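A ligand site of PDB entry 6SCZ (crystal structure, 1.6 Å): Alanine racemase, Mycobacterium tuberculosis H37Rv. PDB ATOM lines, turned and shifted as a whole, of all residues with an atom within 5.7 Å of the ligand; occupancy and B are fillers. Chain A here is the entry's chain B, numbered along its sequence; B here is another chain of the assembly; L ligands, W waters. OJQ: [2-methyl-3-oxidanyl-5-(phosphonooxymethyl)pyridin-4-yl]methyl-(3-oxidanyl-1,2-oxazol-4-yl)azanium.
A ring nitrogen (ND1) of His 175 sits close to a nitrogen (N1) of the ligand. The backbone NH of Ser 216 sits at hydrogen-bond distance from an oxygen (O1P) of the ligand, at 2.8 Å. NZ of Lys 45 sits at hydrogen-bond distance from O1 of the ligand (3.0 Å). The guanidinium group (NE) of Arg 231 is in hydrogen-bond range of a nitrogen (N1) of the ligand, 2.9 Å away. An oxygen (O) of the ligand lies within hydrogen-bond range of the guanidinium group of Arg 143 (3.4 Å). The side-chain hydroxyl (OH) of Tyr 274 of chain B is in hydrogen-bond range of an oxygen (O) of the ligand (2.5 Å). The backbone NH (N) of Met 322 of chain B sits at hydrogen-bond distance from a nitrogen (ND) of the ligand, 3.0 Å away. An oxygen (O1P) of the ligand lies within hydrogen-bond range of the backbone NH (N) of Gly 233, at 2.9 Å. OH of Tyr 49 lies within hydrogen-bond range of O2P of the ligand (2.6 Å). The side-chain hydroxyl of Tyr 367 is in hydrogen-bond range of an oxygen (O3P) of the ligand, 2.6 Å away. An oxygen (O2P) of the ligand is in hydrogen-bond range of the backbone NH (N) of Ile 234, at 2.7 Å. The side-chain hydroxyl (OH) of Tyr 293 of chain B lies within hydrogen-bond range of an oxygen (OG) of the ligand, at 3.1 Å. OG of Ser 216 is in hydrogen-bond range of O1P of the ligand, 2.7 Å away.
The guanidinium group (NE) of Arg 143 sits close to the side-chain amide oxygen (OE1) of Gln 324 of chain B (3.4 Å). The backbone carbonyl oxygen of Gln 324 of chain B sits close to the side-chain sulfur of Cys 321 of chain B (3.7 Å). OG of Ser 216 lies within hydrogen-bond range of N of Ile 234 (3.4 Å). NH1 of Arg 143 lies within hydrogen-bond range of SG of Cys 321 of chain B (3.2 Å). The backbone NH of Val 43 is in hydrogen-bond range of the backbone carbonyl oxygen of Pro 232 (3.0 Å). The guanidinium group (NH1) of Arg 143 is in hydrogen-bond range of the side-chain hydroxyl (OH) of Tyr 274 of chain B, at 3.4 Å. O of Cys 321 of chain B is in hydrogen-bond range of N of Tyr 293 of chain B (3.0 Å). O of Met 322 of chain B sits at hydrogen-bond distance from N of Tyr 293 of chain B.
Val 43 touches the ligand (CG2 to C6, 3.8 Å). Trp 91 touches the ligand. Met 173 touches the ligand (CE to C2A, 3.9 Å). Asn 215 touches the ligand (CB to O1P, 3.7 Å). Pro 232 touches the ligand. Cys 321 of chain B touches the ligand (CB to O, 3.5 Å). Hydrophobic or aromatic side chains that line the ligand: Val 43, Tyr 49, Trp 91, Met 173, His 175, Ile 234, Tyr 367, Tyr 274 of chain B and Met 322 of chain B.
Water W1 lies within hydrogen-bond range of ND of the ligand (2.7 Å) and OH of Tyr 293 of chain B (2.8 Å). Water W2 bridges O3P of the ligand (2.8 Å) and NE2 of His 175 (3.4 Å).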
ATOM      1  N   VAL A  43     -14.761  21.839  28.464  1.00  0.00           N
ATOM      2  CA  VAL A  43     -15.833  22.675  27.939  1.00  0.00           C
ATOM      3  C   VAL A  43     -16.681  23.182  29.096  1.00  0.00           C
ATOM      4  O   VAL A  43     -17.328  22.411  29.811  1.00  0.00           O
ATOM      5  CB  VAL A  43     -16.691  21.914  26.921  1.00  0.00           C
ATOM      6  CG1 VAL A  43     -17.814  22.824  26.412  1.00  0.00           C
ATOM      7  CG2 VAL A  43     -15.805  21.426  25.783  1.00  0.00           C
ATOM      8  N   LYS A  45     -18.843  26.033  28.755  1.00  0.00           N
ATOM      9  CA  LYS A  45     -19.906  26.908  28.291  1.00  0.00           C
ATOM     10  C   LYS A  45     -21.138  26.762  29.181  1.00  0.00           C
ATOM     11  O   LYS A  45     -21.280  25.817  29.948  1.00  0.00           O
ATOM     12  CB  LYS A  45     -20.257  26.606  26.831  1.00  0.00           C
ATOM     13  CG  LYS A  45     -21.008  25.309  26.589  1.00  0.00           C
ATOM     14  CD  LYS A  45     -21.040  24.980  25.091  1.00  0.00           C
ATOM     15  CE  LYS A  45     -22.372  24.390  24.673  1.00  0.00           C
ATOM     16  NZ  LYS A  45     -22.475  24.229  23.181  1.00  0.00           N
ATOM     17  N   TYR A  49     -22.005  24.326  32.440  1.00  0.00           N
ATOM     18  CA  TYR A  49     -23.181  23.457  32.404  1.00  0.00           C
ATOM     19  C   TYR A  49     -23.955  23.591  33.717  1.00  0.00           C
ATOM     20  O   TYR A  49     -24.396  22.605  34.313  1.00  0.00           O
ATOM     21  CB  TYR A  49     -22.819  21.982  32.156  1.00  0.00           C
ATOM     22  CG  TYR A  49     -22.369  21.550  30.774  1.00  0.00           C
ATOM     23  CD1 TYR A  49     -21.801  22.438  29.889  1.00  0.00           C
ATOM     24  CD2 TYR A  49     -22.466  20.228  30.382  1.00  0.00           C
ATOM     25  CE1 TYR A  49     -21.366  22.019  28.631  1.00  0.00           C
ATOM     26  CE2 TYR A  49     -22.034  19.792  29.141  1.00  0.00           C
ATOM     27  CZ  TYR A  49     -21.465  20.695  28.272  1.00  0.00           C
ATOM     28  OH  TYR A  49     -21.036  20.297  27.026  1.00  0.00           O
ATOM     29  N   TRP A  91     -16.457  29.562  20.073  1.00  0.00           N
ATOM     30  CA  TRP A  91     -16.777  29.063  18.743  1.00  0.00           C
ATOM     31  C   TRP A  91     -18.175  29.395  18.225  1.00  0.00           C
ATOM     32  O   TRP A  91     -18.513  28.934  17.129  1.00  0.00           O
ATOM     33  CB  TRP A  91     -16.592  27.539  18.686  1.00  0.00           C
ATOM     34  CG  TRP A  91     -17.308  26.815  19.754  1.00  0.00           C
ATOM     35  CD1 TRP A  91     -18.657  26.721  19.936  1.00  0.00           C
ATOM     36  CD2 TRP A  91     -16.712  26.085  20.829  1.00  0.00           C
ATOM     37  NE1 TRP A  91     -18.941  25.974  21.047  1.00  0.00           N
ATOM     38  CE2 TRP A  91     -17.761  25.573  21.615  1.00  0.00           C
ATOM     39  CE3 TRP A  91     -15.389  25.799  21.196  1.00  0.00           C
ATOM     40  CZ2 TRP A  91     -17.535  24.793  22.731  1.00  0.00           C
ATOM     41  CZ3 TRP A  91     -15.163  25.019  22.312  1.00  0.00           C
ATOM     42  CH2 TRP A  91     -16.239  24.528  23.074  1.00  0.00           C
ATOM     43  N   LYS A 136     -13.773  26.082  12.318  1.00  0.00           N
ATOM     44  CA  LYS A 136     -14.794  25.093  12.662  1.00  0.00           C
ATOM     45  C   LYS A 136     -15.437  24.612  11.373  1.00  0.00           C
ATOM     46  O   LYS A 136     -16.048  25.405  10.653  1.00  0.00           O
ATOM     47  CB  LYS A 136     -15.850  25.712  13.576  1.00  0.00           C
ATOM     48  CG  LYS A 136     -16.864  24.720  14.185  1.00  0.00           C
ATOM     49  CD  LYS A 136     -17.617  25.376  15.382  1.00  0.00           C
ATOM     50  CE  LYS A 136     -18.442  24.348  16.166  1.00  0.00           C
ATOM     51  NZ  LYS A 136     -19.700  23.991  15.443  1.00  0.00           N
ATOM     52  N   ARG A 143     -24.833  22.260  11.414  1.00  0.00           N
ATOM     53  CA  ARG A 143     -25.158  23.508  12.090  1.00  0.00           C
ATOM     54  C   ARG A 143     -24.284  24.624  11.518  1.00  0.00           C
ATOM     55  O   ARG A 143     -24.440  24.964  10.344  1.00  0.00           O
ATOM     56  CB  ARG A 143     -25.008  23.354  13.601  1.00  0.00           C
ATOM     57  CG  ARG A 143     -25.932  22.284  14.146  1.00  0.00           C
ATOM     58  CD  ARG A 143     -25.879  22.208  15.675  1.00  0.00           C
ATOM     59  NE  ARG A 143     -24.507  22.219  16.188  1.00  0.00           N
ATOM     60  CZ  ARG A 143     -24.188  22.192  17.474  1.00  0.00           C
ATOM     61  NH1 ARG A 143     -25.147  22.145  18.397  1.00  0.00           N
ATOM     62  NH2 ARG A 143     -22.926  22.217  17.855  1.00  0.00           N
ATOM     63  N   MET A 173     -11.326  22.324  14.024  1.00  0.00           N
ATOM     64  CA  MET A 173     -12.258  21.652  14.916  1.00  0.00           C
ATOM     65  C   MET A 173     -13.528  21.263  14.183  1.00  0.00           C
ATOM     66  O   MET A 173     -13.921  21.894  13.191  1.00  0.00           O
ATOM     67  CB  MET A 173     -12.599  22.537  16.136  1.00  0.00           C
ATOM     68  CG  MET A 173     -13.548  23.687  15.838  1.00  0.00           C
ATOM     69  SD  MET A 173     -13.949  24.680  17.277  1.00  0.00           S
ATOM     70  CE  MET A 173     -15.065  23.578  18.146  1.00  0.00           C
ATOM     71  N   HIS A 175     -17.446  18.845  15.312  1.00  0.00           N
ATOM     72  CA  HIS A 175     -18.227  18.337  16.434  1.00  0.00           C
ATOM     73  C   HIS A 175     -19.081  17.167  15.970  1.00  0.00           C
ATOM     74  O   HIS A 175     -19.590  17.146  14.850  1.00  0.00           O
ATOM     75  CB  HIS A 175     -19.086  19.454  17.039  1.00  0.00           C
ATOM     76  CG  HIS A 175     -19.661  19.149  18.391  1.00  0.00           C
ATOM     77  ND1 HIS A 175     -18.939  18.598  19.433  1.00  0.00           N
ATOM     78  CD2 HIS A 175     -20.903  19.367  18.875  1.00  0.00           C
ATOM     79  CE1 HIS A 175     -19.717  18.496  20.494  1.00  0.00           C
ATOM     80  NE2 HIS A 175     -20.916  18.955  20.184  1.00  0.00           N
ATOM     81  N   ALA A 179     -23.796  12.597  20.656  1.00  0.00           N
ATOM     82  CA  ALA A 179     -23.187  12.812  21.963  1.00  0.00           C
ATOM     83  C   ALA A 179     -23.142  11.544  22.806  1.00  0.00           C
ATOM     84  O   ALA A 179     -22.395  11.498  23.794  1.00  0.00           O
ATOM     85  CB  ALA A 179     -23.937  13.915  22.733  1.00  0.00           C
ATOM     86  N   SER A 214     -13.282  15.383  19.304  1.00  0.00           N
ATOM     87  CA  SER A 214     -13.879  14.485  20.288  1.00  0.00           C
ATOM     88  C   SER A 214     -14.609  15.226  21.410  1.00  0.00           C
ATOM     89  O   SER A 214     -14.008  16.073  22.090  1.00  0.00           O
ATOM     90  CB  SER A 214     -12.795  13.597  20.902  1.00  0.00           C
ATOM     91  OG  SER A 214     -12.006  12.971  19.906  1.00  0.00           O
ATOM     92  N   ASN A 215     -15.863  14.852  21.625  1.00  0.00           N
ATOM     93  CA  ASN A 215     -16.643  15.195  22.817  1.00  0.00           C
ATOM     94  C   ASN A 215     -16.345  14.169  23.915  1.00  0.00           C
ATOM     95  O   ASN A 215     -15.457  13.331  23.778  1.00  0.00           O
ATOM     96  CB  ASN A 215     -18.135  15.249  22.466  1.00  0.00           C
ATOM     97  CG  ASN A 215     -18.649  13.966  21.850  1.00  0.00           C
ATOM     98  OD1 ASN A 215     -17.997  12.933  21.901  1.00  0.00           O
ATOM     99  ND2 ASN A 215     -19.846  14.021  21.271  1.00  0.00           N
ATOM    100  N   SER A 216     -17.121  14.209  25.005  1.00  0.00           N
ATOM    101  CA  SER A 216     -16.920  13.238  26.088  1.00  0.00           C
ATOM    102  C   SER A 216     -17.092  11.800  25.611  1.00  0.00           C
ATOM    103  O   SER A 216     -16.284  10.932  25.945  1.00  0.00           O
ATOM    104  CB  SER A 216     -17.892  13.515  27.235  1.00  0.00           C
ATOM    105  OG  SER A 216     -17.617  14.759  27.841  1.00  0.00           O
ATOM    106  N   SER A 217     -18.166  11.528  24.859  1.00  0.00           N
ATOM    107  CA  SER A 217     -18.450  10.168  24.409  1.00  0.00           C
ATOM    108  C   SER A 217     -17.313   9.619  23.566  1.00  0.00           C
ATOM    109  O   SER A 217     -16.881   8.486  23.755  1.00  0.00           O
ATOM    110  CB  SER A 217     -19.755  10.137  23.619  1.00  0.00           C
ATOM    111  OG  SER A 217     -19.784   9.012  22.727  1.00  0.00           O
ATOM    112  N   ARG A 231     -12.227  17.477  23.660  1.00  0.00           N
ATOM    113  CA  ARG A 231     -13.070  18.582  24.108  1.00  0.00           C
ATOM    114  C   ARG A 231     -14.261  18.075  24.936  1.00  0.00           C
ATOM    115  O   ARG A 231     -15.419  18.250  24.543  1.00  0.00           O
ATOM    116  CB  ARG A 231     -13.618  19.364  22.909  1.00  0.00           C
ATOM    117  CG  ARG A 231     -12.721  20.311  22.235  1.00  0.00           C
ATOM    118  CD  ARG A 231     -13.516  21.323  21.351  1.00  0.00           C
ATOM    119  NE  ARG A 231     -14.720  20.741  20.752  1.00  0.00           N
ATOM    120  CZ  ARG A 231     -14.737  20.041  19.608  1.00  0.00           C
ATOM    121  NH1 ARG A 231     -13.610  19.863  18.914  1.00  0.00           N
ATOM    122  NH2 ARG A 231     -15.867  19.515  19.172  1.00  0.00           N
ATOM    123  N   PRO A 232     -14.001  17.452  26.079  1.00  0.00           N
ATOM    124  CA  PRO A 232     -15.117  16.940  26.887  1.00  0.00           C
ATOM    125  C   PRO A 232     -15.832  18.022  27.694  1.00  0.00           C
ATOM    126  O   PRO A 232     -15.200  18.870  28.323  1.00  0.00           O
ATOM    127  CB  PRO A 232     -14.431  15.940  27.827  1.00  0.00           C
ATOM    128  CG  PRO A 232     -13.064  16.470  27.969  1.00  0.00           C
ATOM    129  CD  PRO A 232     -12.702  17.075  26.645  1.00  0.00           C
ATOM    130  N   GLY A 233     -17.161  17.958  27.669  1.00  0.00           N
ATOM    131  CA  GLY A 233     -17.979  18.747  28.582  1.00  0.00           C
ATOM    132  C   GLY A 233     -18.660  17.881  29.616  1.00  0.00           C
ATOM    133  O   GLY A 233     -18.255  17.873  30.787  1.00  0.00           O
ATOM    134  N   ILE A 234     -19.680  17.123  29.207  1.00  0.00           N
ATOM    135  CA  ILE A 234     -20.588  16.491  30.152  1.00  0.00           C
ATOM    136  C   ILE A 234     -19.828  15.611  31.151  1.00  0.00           C
ATOM    137  O   ILE A 234     -20.151  15.573  32.343  1.00  0.00           O
ATOM    138  CB  ILE A 234     -21.653  15.705  29.375  1.00  0.00           C
ATOM    139  CG1 ILE A 234     -22.798  15.260  30.260  1.00  0.00           C
ATOM    140  CG2 ILE A 234     -21.049  14.487  28.652  1.00  0.00           C
ATOM    141  CD1 ILE A 234     -23.557  16.433  30.891  1.00  0.00           C
ATOM    142  N   ALA A 235     -18.770  14.932  30.700  1.00  0.00           N
ATOM    143  CA  ALA A 235     -18.051  14.027  31.583  1.00  0.00           C
ATOM    144  C   ALA A 235     -17.249  14.775  32.642  1.00  0.00           C
ATOM    145  O   ALA A 235     -16.990  14.216  33.714  1.00  0.00           O
ATOM    146  CB  ALA A 235     -17.135  13.120  30.756  1.00  0.00           C
ATOM    147  N   TYR A 367     -27.872  16.641  30.589  1.00  0.00           N
ATOM    148  CA  TYR A 367     -27.395  17.982  30.255  1.00  0.00           C
ATOM    149  C   TYR A 367     -28.430  19.047  30.625  1.00  0.00           C
ATOM    150  O   TYR A 367     -28.091  20.106  31.154  1.00  0.00           O
ATOM    151  CB  TYR A 367     -27.142  18.120  28.747  1.00  0.00           C
ATOM    152  CG  TYR A 367     -26.072  17.301  28.072  1.00  0.00           C
ATOM    153  CD1 TYR A 367     -26.254  15.946  27.833  1.00  0.00           C
ATOM    154  CD2 TYR A 367     -24.933  17.896  27.605  1.00  0.00           C
ATOM    155  CE1 TYR A 367     -25.292  15.218  27.158  1.00  0.00           C
ATOM    156  CE2 TYR A 367     -23.964  17.172  26.918  1.00  0.00           C
ATOM    157  CZ  TYR A 367     -24.148  15.820  26.721  1.00  0.00           C
ATOM    158  OH  TYR A 367     -23.220  15.055  26.056  1.00  0.00           O
ATOM    159  N   TYR B 274     -28.159  16.850  16.654  1.00  0.00           N
ATOM    160  CA  TYR B 274     -27.689  15.613  17.276  1.00  0.00           C
ATOM    161  C   TYR B 274     -28.610  14.461  16.926  1.00  0.00           C
ATOM    162  O   TYR B 274     -29.837  14.600  16.931  1.00  0.00           O
ATOM    163  CB  TYR B 274     -27.612  15.761  18.791  1.00  0.00           C
ATOM    164  CG  TYR B 274     -26.592  16.796  19.194  1.00  0.00           C
ATOM    165  CD1 TYR B 274     -25.255  16.647  18.838  1.00  0.00           C
ATOM    166  CD2 TYR B 274     -26.963  17.922  19.893  1.00  0.00           C
ATOM    167  CE1 TYR B 274     -24.331  17.587  19.179  1.00  0.00           C
ATOM    168  CE2 TYR B 274     -26.039  18.887  20.234  1.00  0.00           C
ATOM    169  CZ  TYR B 274     -24.726  18.722  19.859  1.00  0.00           C
ATOM    170  OH  TYR B 274     -23.803  19.665  20.209  1.00  0.00           O
ATOM    171  N   TYR B 293     -31.683  25.046  25.396  1.00  0.00           N
ATOM    172  CA  TYR B 293     -32.377  24.660  26.611  1.00  0.00           C
ATOM    173  C   TYR B 293     -31.713  25.228  27.866  1.00  0.00           C
ATOM    174  O   TYR B 293     -32.403  25.383  28.877  1.00  0.00           O
ATOM    175  CB  TYR B 293     -32.557  23.135  26.717  1.00  0.00           C
ATOM    176  CG  TYR B 293     -31.329  22.265  26.602  1.00  0.00           C
ATOM    177  CD1 TYR B 293     -30.425  22.178  27.653  1.00  0.00           C
ATOM    178  CD2 TYR B 293     -31.110  21.484  25.473  1.00  0.00           C
ATOM    179  CE1 TYR B 293     -29.304  21.369  27.561  1.00  0.00           C
ATOM    180  CE2 TYR B 293     -29.992  20.663  25.375  1.00  0.00           C
ATOM    181  CZ  TYR B 293     -29.087  20.622  26.418  1.00  0.00           C
ATOM    182  OH  TYR B 293     -27.979  19.833  26.327  1.00  0.00           O
ATOM    183  N   CYS B 321     -30.486  22.140  21.102  1.00  0.00           N
ATOM    184  CA  CYS B 321     -29.206  21.967  21.776  1.00  0.00           C
ATOM    185  C   CYS B 321     -29.145  22.864  23.009  1.00  0.00           C
ATOM    186  O   CYS B 321     -30.075  23.624  23.315  1.00  0.00           O
ATOM    187  CB  CYS B 321     -28.061  22.292  20.821  1.00  0.00           C
ATOM    188  SG  CYS B 321     -28.145  21.409  19.283  1.00  0.00           S
ATOM    189  N   MET B 322     -28.037  22.769  23.745  1.00  0.00           N
ATOM    190  CA  MET B 322     -27.900  23.555  24.970  1.00  0.00           C
ATOM    191  C   MET B 322     -28.012  25.043  24.681  1.00  0.00           C
ATOM    192  O   MET B 322     -28.573  25.796  25.485  1.00  0.00           O
ATOM    193  CB  MET B 322     -26.570  23.258  25.660  1.00  0.00           C
ATOM    194  CG  MET B 322     -26.430  23.893  27.025  1.00  0.00           C
ATOM    195  SD  MET B 322     -24.900  23.398  27.862  1.00  0.00           S
ATOM    196  CE  MET B 322     -25.324  21.734  28.316  1.00  0.00           C
ATOM    197  N   ASP B 323     -27.479  25.494  23.546  1.00  0.00           N
ATOM    198  CA  ASP B 323     -27.370  26.926  23.282  1.00  0.00           C
ATOM    199  C   ASP B 323     -27.835  27.341  21.899  1.00  0.00           C
ATOM    200  O   ASP B 323     -27.609  28.487  21.499  1.00  0.00           O
ATOM    201  CB  ASP B 323     -25.924  27.399  23.515  1.00  0.00           C
ATOM    202  CG  ASP B 323     -24.962  27.003  22.395  1.00  0.00           C
ATOM    203  OD1 ASP B 323     -25.243  26.108  21.576  1.00  0.00           O
ATOM    204  OD2 ASP B 323     -23.883  27.606  22.363  1.00  0.00           O
ATOM    205  N   GLN B 324     -28.538  26.468  21.170  1.00  0.00           N
ATOM    206  CA  GLN B 324     -28.953  26.784  19.803  1.00  0.00           C
ATOM    207  C   GLN B 324     -29.942  25.756  19.292  1.00  0.00           C
ATOM    208  O   GLN B 324     -30.005  24.623  19.778  1.00  0.00           O
ATOM    209  CB  GLN B 324     -27.751  26.834  18.862  1.00  0.00           C
ATOM    210  CG  GLN B 324     -27.052  25.478  18.758  1.00  0.00           C
ATOM    211  CD  GLN B 324     -25.740  25.581  18.042  1.00  0.00           C
ATOM    212  OE1 GLN B 324     -25.670  25.348  16.847  1.00  0.00           O
ATOM    213  NE2 GLN B 324     -24.694  25.957  18.757  1.00  0.00           N
HETATM  214  C3  OJQ L   1     -19.682  21.616  21.955  1.00  0.00           C
HETATM  215  C4  OJQ L   1     -19.813  20.751  23.029  1.00  0.00           C
HETATM  216  C5  OJQ L   1     -18.728  19.965  23.393  1.00  0.00           C
HETATM  217  C6  OJQ L   1     -17.555  20.041  22.666  1.00  0.00           C
HETATM  218  C2  OJQ L   1     -18.495  21.667  21.251  1.00  0.00           C
HETATM  219  N   OJQ L   1     -22.287  20.627  22.963  1.00  0.00           N
HETATM  220  CA  OJQ L   1     -23.535  20.440  23.616  1.00  0.00           C
HETATM  221  C   OJQ L   1     -24.785  20.933  23.009  1.00  0.00           C
HETATM  222  O   OJQ L   1     -24.797  21.481  21.662  1.00  0.00           O
HETATM  223  CB  OJQ L   1     -23.941  20.046  24.867  1.00  0.00           C
HETATM  224  OG  OJQ L   1     -25.304  20.198  24.878  1.00  0.00           O
HETATM  225  ND  OJQ L   1     -25.840  20.724  23.777  1.00  0.00           N
HETATM  226  C2A OJQ L   1     -18.340  22.564  20.058  1.00  0.00           C
HETATM  227  C4A OJQ L   1     -21.099  20.698  23.839  1.00  0.00           C
HETATM  228  C5A OJQ L   1     -18.760  19.026  24.580  1.00  0.00           C
HETATM  229  N1  OJQ L   1     -17.463  20.881  21.629  1.00  0.00           N
HETATM  230  O1  OJQ L   1     -20.682  22.390  21.565  1.00  0.00           O
HETATM  231  O1P OJQ L   1     -18.784  16.259  25.940  1.00  0.00           O
HETATM  232  O2P OJQ L   1     -20.653  17.766  26.720  1.00  0.00           O
HETATM  233  O3P OJQ L   1     -21.074  16.041  24.913  1.00  0.00           O
HETATM  234  O4P OJQ L   1     -19.692  17.996  24.363  1.00  0.00           O
HETATM  235  P   OJQ L   1     -20.069  16.975  25.542  1.00  0.00           P
HETATM  236  O   HOH W   1     -27.623  18.739  23.806  1.00  0.00           O
HETATM  237  O   HOH W   2     -22.421  17.254  22.721  1.00  0.00           O
HETATM  238  O   HOH W   3     -20.277  13.374  24.639  1.00  0.00           O
